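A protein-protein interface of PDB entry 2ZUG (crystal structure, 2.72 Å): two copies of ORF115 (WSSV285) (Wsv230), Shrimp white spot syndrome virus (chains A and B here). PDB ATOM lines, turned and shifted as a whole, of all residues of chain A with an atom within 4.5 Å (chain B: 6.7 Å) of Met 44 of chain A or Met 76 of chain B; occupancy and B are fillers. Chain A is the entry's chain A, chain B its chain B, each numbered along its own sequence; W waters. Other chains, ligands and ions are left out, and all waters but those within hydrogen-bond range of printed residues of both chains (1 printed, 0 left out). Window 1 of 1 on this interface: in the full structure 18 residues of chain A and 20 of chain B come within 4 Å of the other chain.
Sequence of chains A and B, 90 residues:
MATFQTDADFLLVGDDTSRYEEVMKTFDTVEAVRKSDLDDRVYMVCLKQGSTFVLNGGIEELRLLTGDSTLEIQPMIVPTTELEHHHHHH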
ATOM      1  N   PHE A  10     -18.083 -29.959   4.431  1.00  0.00           N
ATOM      2  CA  PHE A  10     -16.928 -29.274   3.896  1.00  0.00           C
ATOM      3  C   PHE A  10     -16.840 -27.880   4.468  1.00  0.00           C
ATOM      4  O   PHE A  10     -17.669 -27.495   5.280  1.00  0.00           O
ATOM      5  CB  PHE A  10     -17.048 -29.224   2.371  1.00  0.00           C
ATOM      6  CG  PHE A  10     -18.248 -28.416   1.884  1.00  0.00           C
ATOM      7  CD1 PHE A  10     -18.227 -27.024   1.916  1.00  0.00           C
ATOM      8  CD2 PHE A  10     -19.411 -29.056   1.437  1.00  0.00           C
ATOM      9  CE1 PHE A  10     -19.335 -26.292   1.520  1.00  0.00           C
ATOM     10  CE2 PHE A  10     -20.536 -28.322   1.035  1.00  0.00           C
ATOM     11  CZ  PHE A  10     -20.496 -26.948   1.075  1.00  0.00           C
ATOM     12  N   LEU A  11     -15.851 -27.115   4.022  1.00  0.00           N
ATOM     13  CA  LEU A  11     -15.690 -25.771   4.543  1.00  0.00           C
ATOM     14  C   LEU A  11     -15.741 -24.687   3.484  1.00  0.00           C
ATOM     15  O   LEU A  11     -15.464 -24.923   2.314  1.00  0.00           O
ATOM     16  CB  LEU A  11     -14.353 -25.646   5.276  1.00  0.00           C
ATOM     17  CG  LEU A  11     -13.929 -26.716   6.280  1.00  0.00           C
ATOM     18  CD1 LEU A  11     -12.476 -26.477   6.627  1.00  0.00           C
ATOM     19  CD2 LEU A  11     -14.832 -26.687   7.513  1.00  0.00           C
ATOM     20  N   ALA A  32     -26.769 -27.598   8.425  1.00  0.00           N
ATOM     21  CA  ALA A  32     -26.377 -26.516   9.316  1.00  0.00           C
ATOM     22  C   ALA A  32     -25.078 -25.911   8.848  1.00  0.00           C
ATOM     23  O   ALA A  32     -24.369 -26.470   8.000  1.00  0.00           O
ATOM     24  CB  ALA A  32     -26.236 -27.013  10.749  1.00  0.00           C
ATOM     25  N   VAL A  33     -24.754 -24.773   9.430  1.00  0.00           N
ATOM     26  CA  VAL A  33     -23.546 -24.067   9.064  1.00  0.00           C
ATOM     27  C   VAL A  33     -22.948 -23.486  10.345  1.00  0.00           C
ATOM     28  O   VAL A  33     -23.698 -23.116  11.249  1.00  0.00           O
ATOM     29  CB  VAL A  33     -23.929 -23.008   8.017  1.00  0.00           C
ATOM     30  CG1 VAL A  33     -23.296 -21.697   8.308  1.00  0.00           C
ATOM     31  CG2 VAL A  33     -23.529 -23.519   6.645  1.00  0.00           C
ATOM     32  N   ARG A  34     -21.620 -23.417  10.461  1.00  0.00           N
ATOM     33  CA  ARG A  34     -21.033 -22.894  11.711  1.00  0.00           C
ATOM     34  C   ARG A  34     -19.717 -22.195  11.489  1.00  0.00           C
ATOM     35  O   ARG A  34     -18.828 -22.775  10.878  1.00  0.00           O
ATOM     36  CB  ARG A  34     -20.788 -24.043  12.703  1.00  0.00           C
ATOM     37  CG  ARG A  34     -20.995 -23.685  14.154  1.00  0.00           C
ATOM     38  CD  ARG A  34     -20.689 -24.878  15.059  1.00  0.00           C
ATOM     39  NE  ARG A  34     -21.037 -24.613  16.460  1.00  0.00           N
ATOM     40  CZ  ARG A  34     -22.267 -24.315  16.873  1.00  0.00           C
ATOM     41  NH1 ARG A  34     -23.261 -24.245  15.988  1.00  0.00           N
ATOM     42  NH2 ARG A  34     -22.512 -24.087  18.155  1.00  0.00           N
ATOM     43  N   LEU A  38     -11.786 -20.949  15.621  1.00  0.00           N
ATOM     44  CA  LEU A  38     -10.385 -20.774  15.300  1.00  0.00           C
ATOM     45  C   LEU A  38     -10.027 -19.733  14.253  1.00  0.00           C
ATOM     46  O   LEU A  38      -8.953 -19.143  14.322  1.00  0.00           O
ATOM     47  CB  LEU A  38      -9.792 -22.079  14.794  1.00  0.00           C
ATOM     48  CG  LEU A  38      -9.797 -23.273  15.705  1.00  0.00           C
ATOM     49  CD1 LEU A  38      -9.075 -24.409  15.031  1.00  0.00           C
ATOM     50  CD2 LEU A  38      -9.146 -22.869  16.991  1.00  0.00           C
ATOM     51  N   VAL A  42     -13.402 -18.951   8.191  1.00  0.00           N
ATOM     52  CA  VAL A  42     -13.915 -20.318   8.039  1.00  0.00           C
ATOM     53  C   VAL A  42     -15.329 -20.609   8.542  1.00  0.00           C
ATOM     54  O   VAL A  42     -15.760 -20.122   9.578  1.00  0.00           O
ATOM     55  CB  VAL A  42     -12.976 -21.361   8.686  1.00  0.00           C
ATOM     56  CG1 VAL A  42     -13.521 -22.785   8.484  1.00  0.00           C
ATOM     57  CG2 VAL A  42     -11.616 -21.271   8.058  1.00  0.00           C
ATOM     58  N   TYR A  43     -16.040 -21.412   7.759  1.00  0.00           N
ATOM     59  CA  TYR A  43     -17.378 -21.879   8.065  1.00  0.00           C
ATOM     60  C   TYR A  43     -17.473 -23.343   7.686  1.00  0.00           C
ATOM     61  O   TYR A  43     -17.050 -23.772   6.597  1.00  0.00           O
ATOM     62  CB  TYR A  43     -18.423 -21.130   7.287  1.00  0.00           C
ATOM     63  CG  TYR A  43     -18.937 -19.932   7.983  1.00  0.00           C
ATOM     64  CD1 TYR A  43     -18.166 -18.780   8.092  1.00  0.00           C
ATOM     65  CD2 TYR A  43     -20.216 -19.926   8.504  1.00  0.00           C
ATOM     66  CE1 TYR A  43     -18.676 -17.630   8.707  1.00  0.00           C
ATOM     67  CE2 TYR A  43     -20.737 -18.795   9.121  1.00  0.00           C
ATOM     68  CZ  TYR A  43     -19.964 -17.657   9.214  1.00  0.00           C
ATOM     69  OH  TYR A  43     -20.503 -16.550   9.809  1.00  0.00           O
ATOM     70  N   MET A  44     -18.021 -24.117   8.609  1.00  0.00           N
ATOM     71  CA  MET A  44     -18.203 -25.520   8.365  1.00  0.00           C
ATOM     72  C   MET A  44     -19.619 -25.636   7.836  1.00  0.00           C
ATOM     73  O   MET A  44     -20.561 -24.974   8.338  1.00  0.00           O
ATOM     74  CB  MET A  44     -18.094 -26.294   9.655  1.00  0.00           C
ATOM     75  CG  MET A  44     -16.833 -26.001  10.461  1.00  0.00           C
ATOM     76  SD  MET A  44     -17.102 -26.284  12.413  1.00  0.00           S
ATOM     77  CE  MET A  44     -17.414 -28.270  12.421  1.00  0.00           C
ATOM     78  N   VAL A  45     -19.756 -26.457   6.803  1.00  0.00           N
ATOM     79  CA  VAL A  45     -21.038 -26.721   6.193  1.00  0.00           C
ATOM     80  C   VAL A  45     -21.279 -28.208   6.371  1.00  0.00           C
ATOM     81  O   VAL A  45     -20.558 -29.043   5.811  1.00  0.00           O
ATOM     82  CB  VAL A  45     -21.018 -26.373   4.690  1.00  0.00           C
ATOM     83  CG1 VAL A  45     -22.360 -26.716   4.044  1.00  0.00           C
ATOM     84  CG2 VAL A  45     -20.689 -24.914   4.524  1.00  0.00           C
ATOM     85  N   CYS A  46     -22.287 -28.532   7.172  1.00  0.00           N
ATOM     86  CA  CYS A  46     -22.630 -29.929   7.429  1.00  0.00           C
ATOM     87  C   CYS A  46     -23.945 -30.211   6.628  1.00  0.00           C
ATOM     88  O   CYS A  46     -24.922 -29.464   6.728  1.00  0.00           O
ATOM     89  CB  CYS A  46     -22.767 -30.179   8.984  1.00  0.00           C
ATOM     90  SG  CYS A  46     -21.741 -29.088  10.209  1.00  0.00           S
ATOM     91  N   ALA B   8     -14.993 -23.465  23.553  1.00  0.00           N
ATOM     92  CA  ALA B   8     -14.873 -23.700  22.130  1.00  0.00           C
ATOM     93  C   ALA B   8     -15.143 -25.100  21.695  1.00  0.00           C
ATOM     94  O   ALA B   8     -14.770 -26.033  22.389  1.00  0.00           O
ATOM     95  CB  ALA B   8     -13.496 -23.300  21.667  1.00  0.00           C
ATOM     96  N   ASP B   9     -15.753 -25.231  20.516  1.00  0.00           N
ATOM     97  CA  ASP B   9     -16.072 -26.523  19.940  1.00  0.00           C
ATOM     98  C   ASP B   9     -14.824 -27.397  19.979  1.00  0.00           C
ATOM     99  O   ASP B   9     -13.723 -26.909  20.085  1.00  0.00           O
ATOM    100  CB  ASP B   9     -16.540 -26.392  18.495  1.00  0.00           C
ATOM    101  CG  ASP B   9     -17.680 -25.391  18.316  1.00  0.00           C
ATOM    102  OD1 ASP B   9     -18.606 -25.315  19.175  1.00  0.00           O
ATOM    103  OD2 ASP B   9     -17.647 -24.683  17.266  1.00  0.00           O
ATOM    104  N   PHE B  10     -14.975 -28.699  19.865  1.00  0.00           N
ATOM    105  CA  PHE B  10     -13.793 -29.506  19.968  1.00  0.00           C
ATOM    106  C   PHE B  10     -14.105 -30.896  19.480  1.00  0.00           C
ATOM    107  O   PHE B  10     -15.256 -31.206  19.220  1.00  0.00           O
ATOM    108  CB  PHE B  10     -13.363 -29.546  21.433  1.00  0.00           C
ATOM    109  CG  PHE B  10     -14.404 -30.143  22.352  1.00  0.00           C
ATOM    110  CD1 PHE B  10     -14.580 -31.533  22.431  1.00  0.00           C
ATOM    111  CD2 PHE B  10     -15.221 -29.317  23.138  1.00  0.00           C
ATOM    112  CE1 PHE B  10     -15.569 -32.089  23.290  1.00  0.00           C
ATOM    113  CE2 PHE B  10     -16.201 -29.856  23.992  1.00  0.00           C
ATOM    114  CZ  PHE B  10     -16.380 -31.244  24.072  1.00  0.00           C
ATOM    115  N   LEU B  11     -13.078 -31.725  19.369  1.00  0.00           N
ATOM    116  CA  LEU B  11     -13.267 -33.085  18.920  1.00  0.00           C
ATOM    117  C   LEU B  11     -13.150 -34.161  20.009  1.00  0.00           C
ATOM    118  O   LEU B  11     -12.560 -33.963  21.048  1.00  0.00           O
ATOM    119  CB  LEU B  11     -12.249 -33.409  17.846  1.00  0.00           C
ATOM    120  CG  LEU B  11     -12.027 -32.411  16.728  1.00  0.00           C
ATOM    121  CD1 LEU B  11     -11.013 -32.989  15.752  1.00  0.00           C
ATOM    122  CD2 LEU B  11     -13.341 -32.139  16.027  1.00  0.00           C
ATOM    123  N   MET B  44     -17.374 -34.431  16.101  1.00  0.00           N
ATOM    124  CA  MET B  44     -17.275 -33.014  16.367  1.00  0.00           C
ATOM    125  C   MET B  44     -18.305 -32.668  17.411  1.00  0.00           C
ATOM    126  O   MET B  44     -19.413 -33.201  17.424  1.00  0.00           O
ATOM    127  CB  MET B  44     -17.536 -32.241  15.106  1.00  0.00           C
ATOM    128  CG  MET B  44     -16.666 -32.738  13.986  1.00  0.00           C
ATOM    129  SD  MET B  44     -17.105 -31.889  12.297  1.00  0.00           S
ATOM    130  CE  MET B  44     -17.619 -33.522  11.272  1.00  0.00           C
ATOM    131  N   VAL B  45     -17.932 -31.782  18.305  1.00  0.00           N
ATOM    132  CA  VAL B  45     -18.839 -31.375  19.329  1.00  0.00           C
ATOM    133  C   VAL B  45     -18.969 -29.879  19.268  1.00  0.00           C
ATOM    134  O   VAL B  45     -18.027 -29.155  19.542  1.00  0.00           O
ATOM    135  CB  VAL B  45     -18.352 -31.837  20.717  1.00  0.00           C
ATOM    136  CG1 VAL B  45     -19.228 -31.252  21.797  1.00  0.00           C
ATOM    137  CG2 VAL B  45     -18.406 -33.346  20.787  1.00  0.00           C
ATOM    138  N   CYS B  46     -20.149 -29.423  18.873  1.00  0.00           N
ATOM    139  CA  CYS B  46     -20.413 -28.000  18.776  1.00  0.00           C
ATOM    140  C   CYS B  46     -21.231 -27.632  20.032  1.00  0.00           C
ATOM    141  O   CYS B  46     -22.163 -28.339  20.397  1.00  0.00           O
ATOM    142  CB  CYS B  46     -21.176 -27.698  17.462  1.00  0.00           C
ATOM    143  SG  CYS B  46     -20.527 -28.536  15.915  1.00  0.00           S
ATOM    144  N   GLN B  74      -9.640 -33.374  21.719  1.00  0.00           N
ATOM    145  CA  GLN B  74      -8.601 -32.665  20.992  1.00  0.00           C
ATOM    146  C   GLN B  74      -9.171 -31.453  20.331  1.00  0.00           C
ATOM    147  O   GLN B  74     -10.346 -31.419  19.996  1.00  0.00           O
ATOM    148  CB  GLN B  74      -8.024 -33.546  19.900  1.00  0.00           C
ATOM    149  CG  GLN B  74      -7.476 -34.862  20.392  1.00  0.00           C
ATOM    150  CD  GLN B  74      -6.793 -35.652  19.286  1.00  0.00           C
ATOM    151  OE1 GLN B  74      -6.365 -35.085  18.259  1.00  0.00           O
ATOM    152  NE2 GLN B  74      -6.676 -36.963  19.488  1.00  0.00           N
ATOM    153  N   PRO B  75      -8.340 -30.434  20.113  1.00  0.00           N
ATOM    154  CA  PRO B  75      -8.854 -29.232  19.459  1.00  0.00           C
ATOM    155  C   PRO B  75      -9.185 -29.458  17.976  1.00  0.00           C
ATOM    156  O   PRO B  75      -8.758 -30.445  17.342  1.00  0.00           O
ATOM    157  CB  PRO B  75      -7.725 -28.236  19.659  1.00  0.00           C
ATOM    158  CG  PRO B  75      -6.504 -29.093  19.654  1.00  0.00           C
ATOM    159  CD  PRO B  75      -6.928 -30.266  20.498  1.00  0.00           C
ATOM    160  N   MET B  76      -9.973 -28.541  17.438  1.00  0.00           N
ATOM    161  CA  MET B  76     -10.354 -28.606  16.047  1.00  0.00           C
ATOM    162  C   MET B  76      -9.225 -27.992  15.240  1.00  0.00           C
ATOM    163  O   MET B  76      -8.553 -27.078  15.678  1.00  0.00           O
ATOM    164  CB  MET B  76     -11.638 -27.827  15.798  1.00  0.00           C
ATOM    165  CG  MET B  76     -12.825 -28.282  16.605  1.00  0.00           C
ATOM    166  SD  MET B  76     -14.441 -27.907  15.592  1.00  0.00           S
ATOM    167  CE  MET B  76     -14.169 -29.285  14.235  1.00  0.00           C
ATOM    168  N   ILE B  77      -9.018 -28.513  14.047  1.00  0.00           N
ATOM    169  CA  ILE B  77      -7.970 -27.992  13.211  1.00  0.00           C
ATOM    170  C   ILE B  77      -8.565 -27.319  11.966  1.00  0.00           C
ATOM    171  O   ILE B  77      -9.536 -27.786  11.363  1.00  0.00           O
ATOM    172  CB  ILE B  77      -6.968 -29.137  12.897  1.00  0.00           C
ATOM    173  CG1 ILE B  77      -5.561 -28.568  12.994  1.00  0.00           C
ATOM    174  CG2 ILE B  77      -7.208 -29.773  11.537  1.00  0.00           C
ATOM    175  CD1 ILE B  77      -5.210 -27.940  14.369  1.00  0.00           C
ATOM    176  N   VAL B  78      -7.999 -26.183  11.608  1.00  0.00           N
ATOM    177  CA  VAL B  78      -8.477 -25.410  10.451  1.00  0.00           C
ATOM    178  C   VAL B  78      -7.321 -25.238   9.436  1.00  0.00           C
ATOM    179  O   VAL B  78      -6.155 -25.118   9.837  1.00  0.00           O
ATOM    180  CB  VAL B  78      -8.982 -24.008  10.921  1.00  0.00           C
ATOM    181  CG1 VAL B  78      -7.914 -22.975  10.729  1.00  0.00           C
ATOM    182  CG2 VAL B  78     -10.210 -23.619  10.202  1.00  0.00           C
HETATM  183  O   HOH W   1     -23.016 -28.735  13.362  1.00  0.00           O
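Among the printed residues, pairs that only touch across the chains: Arg 34 of chain A with Cys 46 of chain B, Leu 38 of chain A with Met 76 of chain B, Val 42 of chain A with Val 78 of chain B, Met 44 of chain A with Met 44 of chain B and Met 44 of chain A with Met 76 of chain B.
Water W1 lies within hydrogen-bond range of the side-chain sulfur (SG) of Cys 46 of chain A (3.4 Å) and the side-chain sulfur (SG) of Cys 46 of chain B (3.6 Å).
The backbone carbonyl oxygen of Arg 34 of chain A sits at hydrogen-bond distance from the backbone NH of Met 44 of chain A.
The guanidinium group (NE) of Arg 34 of chain A is in salt-bridge range of the side-chain carboxylate (OD2) of Asp 9 of chain B, at 3.5 Å.
Phe 10 of chain A touches none of the printed residues of chain B.
Ala 32 of chain A touches none of the printed residues of chain B.
Of the printed residues of chain B, Val 42 of chain A touches Val 78 (3.5 Å).
Of chain B, only Met 44 and Met 76 come within 4 Å of Met 44 of chain A.
Of the printed residues of chain A, Asp 9 of chain B touches Arg 34.
Printed residues of chain A within 4 Å of Met 44 of chain B: Met 44 (3.6 Å).
Of the printed residues of chain A, Cys 46 of chain B touches Arg 34.
Printed residues of chain A within 4 Å of Val 78 of chain B: Val 42 (3.5 Å).
The nearest printed residue of chain B that does not touch Leu 38 of chain A is Val 78 of chain B (4.003 Å).
Met 44 of chain A touches its own counterpart, Met 44 of chain B.
Of the 11 printed residues of chain A, 4 touch a printed residue of chain B.
Printed residues of chain A that touch a printed residue of chain B: Arg 34, Leu 38, Val 42 and Met 44.
Hydrophobic or aromatic side chains of chain A that line the printed part of chain B: Leu 38, Val 42 and Met 44.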
